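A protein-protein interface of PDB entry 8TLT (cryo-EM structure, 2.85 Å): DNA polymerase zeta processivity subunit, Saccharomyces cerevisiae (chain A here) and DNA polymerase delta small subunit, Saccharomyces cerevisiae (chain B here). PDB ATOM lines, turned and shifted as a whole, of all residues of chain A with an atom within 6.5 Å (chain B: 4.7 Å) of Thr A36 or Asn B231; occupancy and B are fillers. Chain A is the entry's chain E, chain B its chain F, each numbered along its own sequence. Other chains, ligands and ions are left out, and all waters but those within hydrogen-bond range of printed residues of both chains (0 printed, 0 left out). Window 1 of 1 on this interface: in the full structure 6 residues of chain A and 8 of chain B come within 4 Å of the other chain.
OG1 of Thr A35 sits close to O of Asn B231 (3.3 Å). N of Thr A36 lies within hydrogen-bond range of O of Asn B231 (2.8 Å). The backbone carbonyl oxygen (O) of Tyr A34 sits close to the backbone carbonyl oxygen (O) of Thr B232.
O of Tyr A37 lies within hydrogen-bond range of OG1 of Thr A35, at 3.3 Å. N of Thr A35 is in hydrogen-bond range of O of Val A46, 3.1 Å away. The backbone carbonyl oxygen of Thr A36 is in hydrogen-bond range of the backbone NH of Leu A42. OG1 of Thr B232 lies within hydrogen-bond range of ND2 of Asn B230, 3.2 Å away. The side-chain amide oxygen (OD1) of Asn B231 lies within hydrogen-bond range of the side-chain hydroxyl (OG) of Ser B286, at 2.5 Å. The backbone carbonyl oxygen (O) of Glu B282 is in hydrogen-bond range of the side-chain hydroxyl (OG) of Ser B286 (3.2 Å).
Among the printed residues, pairs that only touch across the chains: Phe A45 with Asn B231 (3.3 Å), Tyr A37 with Glu B282 (3.4 Å), Tyr A37 with Asn B231 (3.5 Å), Phe A45 with Thr B232 (3.7 Å), Thr A36 with Ile B285 (3.8 Å), Asn A41 with Ile B285 (3.8 Å), Phe A45 with Ser B233 (3.9 Å) and Thr A35 with Thr B232 (3.9 Å).
Of chain B, only Asn B231 and Ile B285 come within 4 Å of Thr A36. Asn B231 touches just these residues of chain A: Thr A35, Thr A36, Tyr A37 and Phe A45. Printed residues of chain A within 4 Å of Thr B232: Tyr A34, Thr A35 and Phe A45. Printed residues of chain A within 4 Å of Ser B233: Phe A45. Of the printed residues of chain B, Phe A45 touches Asn B231 (3.3 Å), Thr B232 (3.7 Å) and Ser B233 (3.9 Å). Of the printed residues of chain B, Asn A41 touches Ile B285. Printed residues of chain A within 4 Å of Glu B282: Tyr A37 (3.4 Å). The nearest printed residue of chain B that does not touch Thr A36 is Thr B232 (5.0 Å). The nearest printed residue of chain B that does not touch Phe A45 is Asn B230 (4.2 Å).
Printed residues of chain B that touch a printed residue of chain A: Asn B231, Thr B232, Ser B233, Glu B282 and Ile B285. Hydrophobic or aromatic side chains of chain B that line the printed part of chain A: Ile B285. Printed residues of chain A that touch a printed residue of chain B: Tyr A34, Thr A35, Thr A36, Tyr A37, Asn A41 and Phe A45. Hydrophobic or aromatic side chains of chain A that line the printed part of chain B: Tyr A37 and Phe A45.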
ATOM      1  N   TYR A  34      16.521   9.652 -12.280  1.00  0.00           N
ATOM      2  CA  TYR A  34      16.391   8.314 -11.719  1.00  0.00           C
ATOM      3  C   TYR A  34      15.377   8.339 -10.583  1.00  0.00           C
ATOM      4  O   TYR A  34      15.526   9.110  -9.629  1.00  0.00           O
ATOM      5  CB  TYR A  34      17.746   7.817 -11.220  1.00  0.00           C
ATOM      6  CG  TYR A  34      18.472   6.935 -12.206  1.00  0.00           C
ATOM      7  CD1 TYR A  34      18.867   7.423 -13.442  1.00  0.00           C
ATOM      8  CD2 TYR A  34      18.761   5.614 -11.902  1.00  0.00           C
ATOM      9  CE1 TYR A  34      19.529   6.620 -14.348  1.00  0.00           C
ATOM     10  CE2 TYR A  34      19.419   4.802 -12.801  1.00  0.00           C
ATOM     11  CZ  TYR A  34      19.801   5.310 -14.023  1.00  0.00           C
ATOM     12  OH  TYR A  34      20.460   4.506 -14.923  1.00  0.00           O
ATOM     13  N   THR A  35      14.347   7.501 -10.678  1.00  0.00           N
ATOM     14  CA  THR A  35      13.262   7.544  -9.711  1.00  0.00           C
ATOM     15  C   THR A  35      12.609   6.176  -9.597  1.00  0.00           C
ATOM     16  O   THR A  35      12.776   5.308 -10.458  1.00  0.00           O
ATOM     17  CB  THR A  35      12.212   8.597 -10.088  1.00  0.00           C
ATOM     18  OG1 THR A  35      11.226   8.682  -9.054  1.00  0.00           O
ATOM     19  CG2 THR A  35      11.534   8.226 -11.397  1.00  0.00           C
ATOM     20  N   THR A  36      11.859   5.999  -8.511  1.00  0.00           N
ATOM     21  CA  THR A  36      11.106   4.781  -8.248  1.00  0.00           C
ATOM     22  C   THR A  36       9.600   4.965  -8.383  1.00  0.00           C
ATOM     23  O   THR A  36       8.905   4.019  -8.760  1.00  0.00           O
ATOM     24  CB  THR A  36      11.445   4.253  -6.843  1.00  0.00           C
ATOM     25  OG1 THR A  36      12.671   3.514  -6.895  1.00  0.00           O
ATOM     26  CG2 THR A  36      10.357   3.349  -6.289  1.00  0.00           C
ATOM     27  N   TYR A  37       9.082   6.165  -8.134  1.00  0.00           N
ATOM     28  CA  TYR A  37       7.657   6.447  -8.251  1.00  0.00           C
ATOM     29  C   TYR A  37       7.419   7.373  -9.437  1.00  0.00           C
ATOM     30  O   TYR A  37       7.994   8.463  -9.503  1.00  0.00           O
ATOM     31  CB  TYR A  37       7.116   7.078  -6.969  1.00  0.00           C
ATOM     32  CG  TYR A  37       5.617   7.250  -6.969  1.00  0.00           C
ATOM     33  CD1 TYR A  37       4.775   6.148  -6.944  1.00  0.00           C
ATOM     34  CD2 TYR A  37       5.043   8.511  -7.013  1.00  0.00           C
ATOM     35  CE1 TYR A  37       3.405   6.299  -6.950  1.00  0.00           C
ATOM     36  CE2 TYR A  37       3.674   8.672  -7.021  1.00  0.00           C
ATOM     37  CZ  TYR A  37       2.860   7.563  -6.987  1.00  0.00           C
ATOM     38  OH  TYR A  37       1.494   7.718  -6.993  1.00  0.00           O
ATOM     39  N   GLN A  38       6.575   6.931 -10.371  1.00  0.00           N
ATOM     40  CA  GLN A  38       6.174   7.722 -11.530  1.00  0.00           C
ATOM     41  C   GLN A  38       4.658   7.557 -11.708  1.00  0.00           C
ATOM     42  O   GLN A  38       4.158   7.113 -12.736  1.00  0.00           O
ATOM     43  CB  GLN A  38       6.978   7.325 -12.772  1.00  0.00           C
ATOM     44  CG  GLN A  38       6.566   7.989 -14.099  1.00  0.00           C
ATOM     45  CD  GLN A  38       6.578   9.512 -14.073  1.00  0.00           C
ATOM     46  OE1 GLN A  38       6.012  10.150 -14.958  1.00  0.00           O
ATOM     47  NE2 GLN A  38       7.273  10.096 -13.103  1.00  0.00           N
ATOM     48  N   PHE A  40       3.239   5.263 -10.309  1.00  0.00           N
ATOM     49  CA  PHE A  40       3.145   3.854  -9.969  1.00  0.00           C
ATOM     50  C   PHE A  40       4.471   3.442  -9.354  1.00  0.00           C
ATOM     51  O   PHE A  40       5.496   4.098  -9.549  1.00  0.00           O
ATOM     52  CB  PHE A  40       2.837   2.986 -11.194  1.00  0.00           C
ATOM     53  CG  PHE A  40       1.415   3.068 -11.660  1.00  0.00           C
ATOM     54  CD1 PHE A  40       0.371   2.782 -10.799  1.00  0.00           C
ATOM     55  CD2 PHE A  40       1.123   3.415 -12.968  1.00  0.00           C
ATOM     56  CE1 PHE A  40      -0.938   2.851 -11.229  1.00  0.00           C
ATOM     57  CE2 PHE A  40      -0.183   3.485 -13.404  1.00  0.00           C
ATOM     58  CZ  PHE A  40      -1.216   3.203 -12.534  1.00  0.00           C
ATOM     59  N   ASN A  41       4.445   2.349  -8.600  1.00  0.00           N
ATOM     60  CA  ASN A  41       5.677   1.791  -8.058  1.00  0.00           C
ATOM     61  C   ASN A  41       6.444   1.107  -9.184  1.00  0.00           C
ATOM     62  O   ASN A  41       5.974   0.116  -9.750  1.00  0.00           O
ATOM     63  CB  ASN A  41       5.364   0.816  -6.926  1.00  0.00           C
ATOM     64  CG  ASN A  41       4.207  -0.106  -7.255  1.00  0.00           C
ATOM     65  N   LEU A  42       7.611   1.646  -9.529  1.00  0.00           N
ATOM     66  CA  LEU A  42       8.408   1.061 -10.594  1.00  0.00           C
ATOM     67  C   LEU A  42       9.253  -0.095 -10.059  1.00  0.00           C
ATOM     68  O   LEU A  42       9.585  -0.132  -8.873  1.00  0.00           O
ATOM     69  CB  LEU A  42       9.309   2.119 -11.226  1.00  0.00           C
ATOM     70  CG  LEU A  42       8.589   3.328 -11.828  1.00  0.00           C
ATOM     71  CD1 LEU A  42       9.569   4.250 -12.526  1.00  0.00           C
ATOM     72  CD2 LEU A  42       7.490   2.887 -12.779  1.00  0.00           C
ATOM     73  N   PRO A  43       9.593  -1.065 -10.915  1.00  0.00           N
ATOM     74  CA  PRO A  43      10.390  -2.208 -10.436  1.00  0.00           C
ATOM     75  C   PRO A  43      11.759  -1.827  -9.895  1.00  0.00           C
ATOM     76  O   PRO A  43      12.228  -2.445  -8.932  1.00  0.00           O
ATOM     77  CB  PRO A  43      10.500  -3.099 -11.682  1.00  0.00           C
ATOM     78  CG  PRO A  43       9.361  -2.692 -12.549  1.00  0.00           C
ATOM     79  CD  PRO A  43       9.186  -1.227 -12.320  1.00  0.00           C
ATOM     80  N   GLN A  44      12.415  -0.832 -10.482  1.00  0.00           N
ATOM     81  CA  GLN A  44      13.749  -0.421 -10.053  1.00  0.00           C
ATOM     82  C   GLN A  44      13.804   1.101 -10.069  1.00  0.00           C
ATOM     83  O   GLN A  44      12.779   1.785 -10.148  1.00  0.00           O
ATOM     84  CB  GLN A  44      14.849  -1.013 -10.948  1.00  0.00           C
ATOM     85  CG  GLN A  44      14.562  -2.368 -11.539  1.00  0.00           C
ATOM     86  CD  GLN A  44      15.258  -2.571 -12.865  1.00  0.00           C
ATOM     87  OE1 GLN A  44      14.646  -2.446 -13.923  1.00  0.00           O
ATOM     88  NE2 GLN A  44      16.546  -2.885 -12.817  1.00  0.00           N
ATOM     89  N   PHE A  45      15.020   1.639  -9.995  1.00  0.00           N
ATOM     90  CA  PHE A  45      15.257   3.070 -10.173  1.00  0.00           C
ATOM     91  C   PHE A  45      15.415   3.368 -11.665  1.00  0.00           C
ATOM     92  O   PHE A  45      16.505   3.616 -12.179  1.00  0.00           O
ATOM     93  CB  PHE A  45      16.481   3.508  -9.380  1.00  0.00           C
ATOM     94  CG  PHE A  45      16.174   3.922  -7.972  1.00  0.00           C
ATOM     95  CD1 PHE A  45      16.153   2.990  -6.951  1.00  0.00           C
ATOM     96  CD2 PHE A  45      15.906   5.244  -7.669  1.00  0.00           C
ATOM     97  CE1 PHE A  45      15.872   3.370  -5.657  1.00  0.00           C
ATOM     98  CE2 PHE A  45      15.622   5.627  -6.377  1.00  0.00           C
ATOM     99  CZ  PHE A  45      15.606   4.689  -5.370  1.00  0.00           C
ATOM    100  N   VAL A  46      14.290   3.317 -12.364  1.00  0.00           N
ATOM    101  CA  VAL A  46      14.287   3.595 -13.806  1.00  0.00           C
ATOM    102  C   VAL A  46      14.402   5.099 -14.026  1.00  0.00           C
ATOM    103  O   VAL A  46      13.755   5.876 -13.302  1.00  0.00           O
ATOM    104  CB  VAL A  46      13.016   3.037 -14.449  1.00  0.00           C
ATOM    105  CG1 VAL A  46      12.945   3.412 -15.919  1.00  0.00           C
ATOM    106  CG2 VAL A  46      12.961   1.529 -14.282  1.00  0.00           C
ATOM    107  N   ARG A  50      11.365  14.213 -17.037  1.00  0.00           N
ATOM    108  CA  ARG A  50      10.541  15.151 -16.290  1.00  0.00           C
ATOM    109  C   ARG A  50       9.784  16.128 -17.180  1.00  0.00           C
ATOM    110  O   ARG A  50       9.093  17.007 -16.657  1.00  0.00           O
ATOM    111  CB  ARG A  50      11.406  15.926 -15.293  1.00  0.00           C
ATOM    112  CG  ARG A  50      12.011  15.062 -14.201  1.00  0.00           C
ATOM    113  CD  ARG A  50      11.006  14.812 -13.093  1.00  0.00           C
ATOM    114  NE  ARG A  50      11.529  13.922 -12.064  1.00  0.00           N
ATOM    115  CZ  ARG A  50      11.280  12.622 -12.001  1.00  0.00           C
ATOM    116  NH1 ARG A  50      10.517  12.021 -12.899  1.00  0.00           N
ATOM    117  NH2 ARG A  50      11.809  11.907 -11.013  1.00  0.00           N
ATOM    118  N   ASN B 230      14.531   8.258   0.066  1.00  0.00           N
ATOM    119  CA  ASN B 230      13.465   8.763  -0.790  1.00  0.00           C
ATOM    120  C   ASN B 230      13.428   7.902  -2.048  1.00  0.00           C
ATOM    121  O   ASN B 230      14.117   6.883  -2.149  1.00  0.00           O
ATOM    122  CB  ASN B 230      13.660  10.254  -1.096  1.00  0.00           C
ATOM    123  CG  ASN B 230      15.028  10.564  -1.667  1.00  0.00           C
ATOM    124  OD1 ASN B 230      15.859   9.676  -1.840  1.00  0.00           O
ATOM    125  ND2 ASN B 230      15.267  11.833  -1.962  1.00  0.00           N
ATOM    126  N   ASN B 231      12.613   8.314  -3.018  1.00  0.00           N
ATOM    127  CA  ASN B 231      12.389   7.545  -4.233  1.00  0.00           C
ATOM    128  C   ASN B 231      13.244   8.025  -5.399  1.00  0.00           C
ATOM    129  O   ASN B 231      13.007   7.615  -6.538  1.00  0.00           O
ATOM    130  CB  ASN B 231      10.911   7.585  -4.620  1.00  0.00           C
ATOM    131  CG  ASN B 231      10.009   7.043  -3.534  1.00  0.00           C
ATOM    132  OD1 ASN B 231      10.359   7.061  -2.355  1.00  0.00           O
ATOM    133  ND2 ASN B 231       8.839   6.558  -3.926  1.00  0.00           N
ATOM    134  N   THR B 232      14.229   8.883  -5.143  1.00  0.00           N
ATOM    135  CA  THR B 232      15.070   9.418  -6.205  1.00  0.00           C
ATOM    136  C   THR B 232      16.558   9.180  -6.010  1.00  0.00           C
ATOM    137  O   THR B 232      17.303   9.265  -6.993  1.00  0.00           O
ATOM    138  CB  THR B 232      14.837  10.928  -6.370  1.00  0.00           C
ATOM    139  OG1 THR B 232      14.570  11.516  -5.092  1.00  0.00           O
ATOM    140  CG2 THR B 232      13.660  11.185  -7.294  1.00  0.00           C
ATOM    141  N   SER B 233      17.020   8.893  -4.798  1.00  0.00           N
ATOM    142  CA  SER B 233      18.441   8.682  -4.551  1.00  0.00           C
ATOM    143  C   SER B 233      18.706   7.207  -4.290  1.00  0.00           C
ATOM    144  O   SER B 233      18.372   6.707  -3.204  1.00  0.00           O
ATOM    145  CB  SER B 233      18.909   9.524  -3.365  1.00  0.00           C
ATOM    146  N   PHE B 273      11.141  13.870   2.430  1.00  0.00           N
ATOM    147  CA  PHE B 273      10.060  14.173   1.504  1.00  0.00           C
ATOM    148  C   PHE B 273       9.567  15.589   1.766  1.00  0.00           C
ATOM    149  O   PHE B 273       9.865  16.193   2.799  1.00  0.00           O
ATOM    150  CB  PHE B 273       8.907  13.174   1.632  1.00  0.00           C
ATOM    151  CG  PHE B 273       9.095  11.924   0.825  1.00  0.00           C
ATOM    152  CD1 PHE B 273       8.890  11.930  -0.544  1.00  0.00           C
ATOM    153  CD2 PHE B 273       9.471  10.741   1.434  1.00  0.00           C
ATOM    154  CE1 PHE B 273       9.064  10.782  -1.287  1.00  0.00           C
ATOM    155  CE2 PHE B 273       9.645   9.592   0.695  1.00  0.00           C
ATOM    156  CZ  PHE B 273       9.441   9.613  -0.667  1.00  0.00           C
ATOM    157  N   GLU B 282       4.449   7.060  -2.492  1.00  0.00           N
ATOM    158  CA  GLU B 282       5.899   7.234  -2.423  1.00  0.00           C
ATOM    159  C   GLU B 282       6.402   7.090  -0.991  1.00  0.00           C
ATOM    160  O   GLU B 282       7.438   6.454  -0.737  1.00  0.00           O
ATOM    161  CB  GLU B 282       6.289   8.596  -2.997  1.00  0.00           C
ATOM    162  CG  GLU B 282       5.170   9.622  -2.987  1.00  0.00           C
ATOM    163  CD  GLU B 282       5.141  10.466  -4.243  1.00  0.00           C
ATOM    164  N   ILE B 285       6.476   3.521  -0.169  1.00  0.00           N
ATOM    165  CA  ILE B 285       7.617   2.840  -0.780  1.00  0.00           C
ATOM    166  C   ILE B 285       8.872   3.044   0.063  1.00  0.00           C
ATOM    167  O   ILE B 285       9.605   2.091   0.373  1.00  0.00           O
ATOM    168  CB  ILE B 285       7.826   3.334  -2.223  1.00  0.00           C
ATOM    169  CG1 ILE B 285       6.743   2.775  -3.144  1.00  0.00           C
ATOM    170  CG2 ILE B 285       9.203   2.946  -2.727  1.00  0.00           C
ATOM    171  CD1 ILE B 285       6.703   3.439  -4.498  1.00  0.00           C
ATOM    172  N   SER B 286       9.130   4.292   0.459  1.00  0.00           N
ATOM    173  CA  SER B 286      10.312   4.572   1.271  1.00  0.00           C
ATOM    174  C   SER B 286      10.221   3.896   2.636  1.00  0.00           C
ATOM    175  O   SER B 286      11.220   3.376   3.154  1.00  0.00           O
ATOM    176  CB  SER B 286      10.495   6.079   1.422  1.00  0.00           C
ATOM    177  OG  SER B 286      10.491   6.706   0.155  1.00  0.00           O
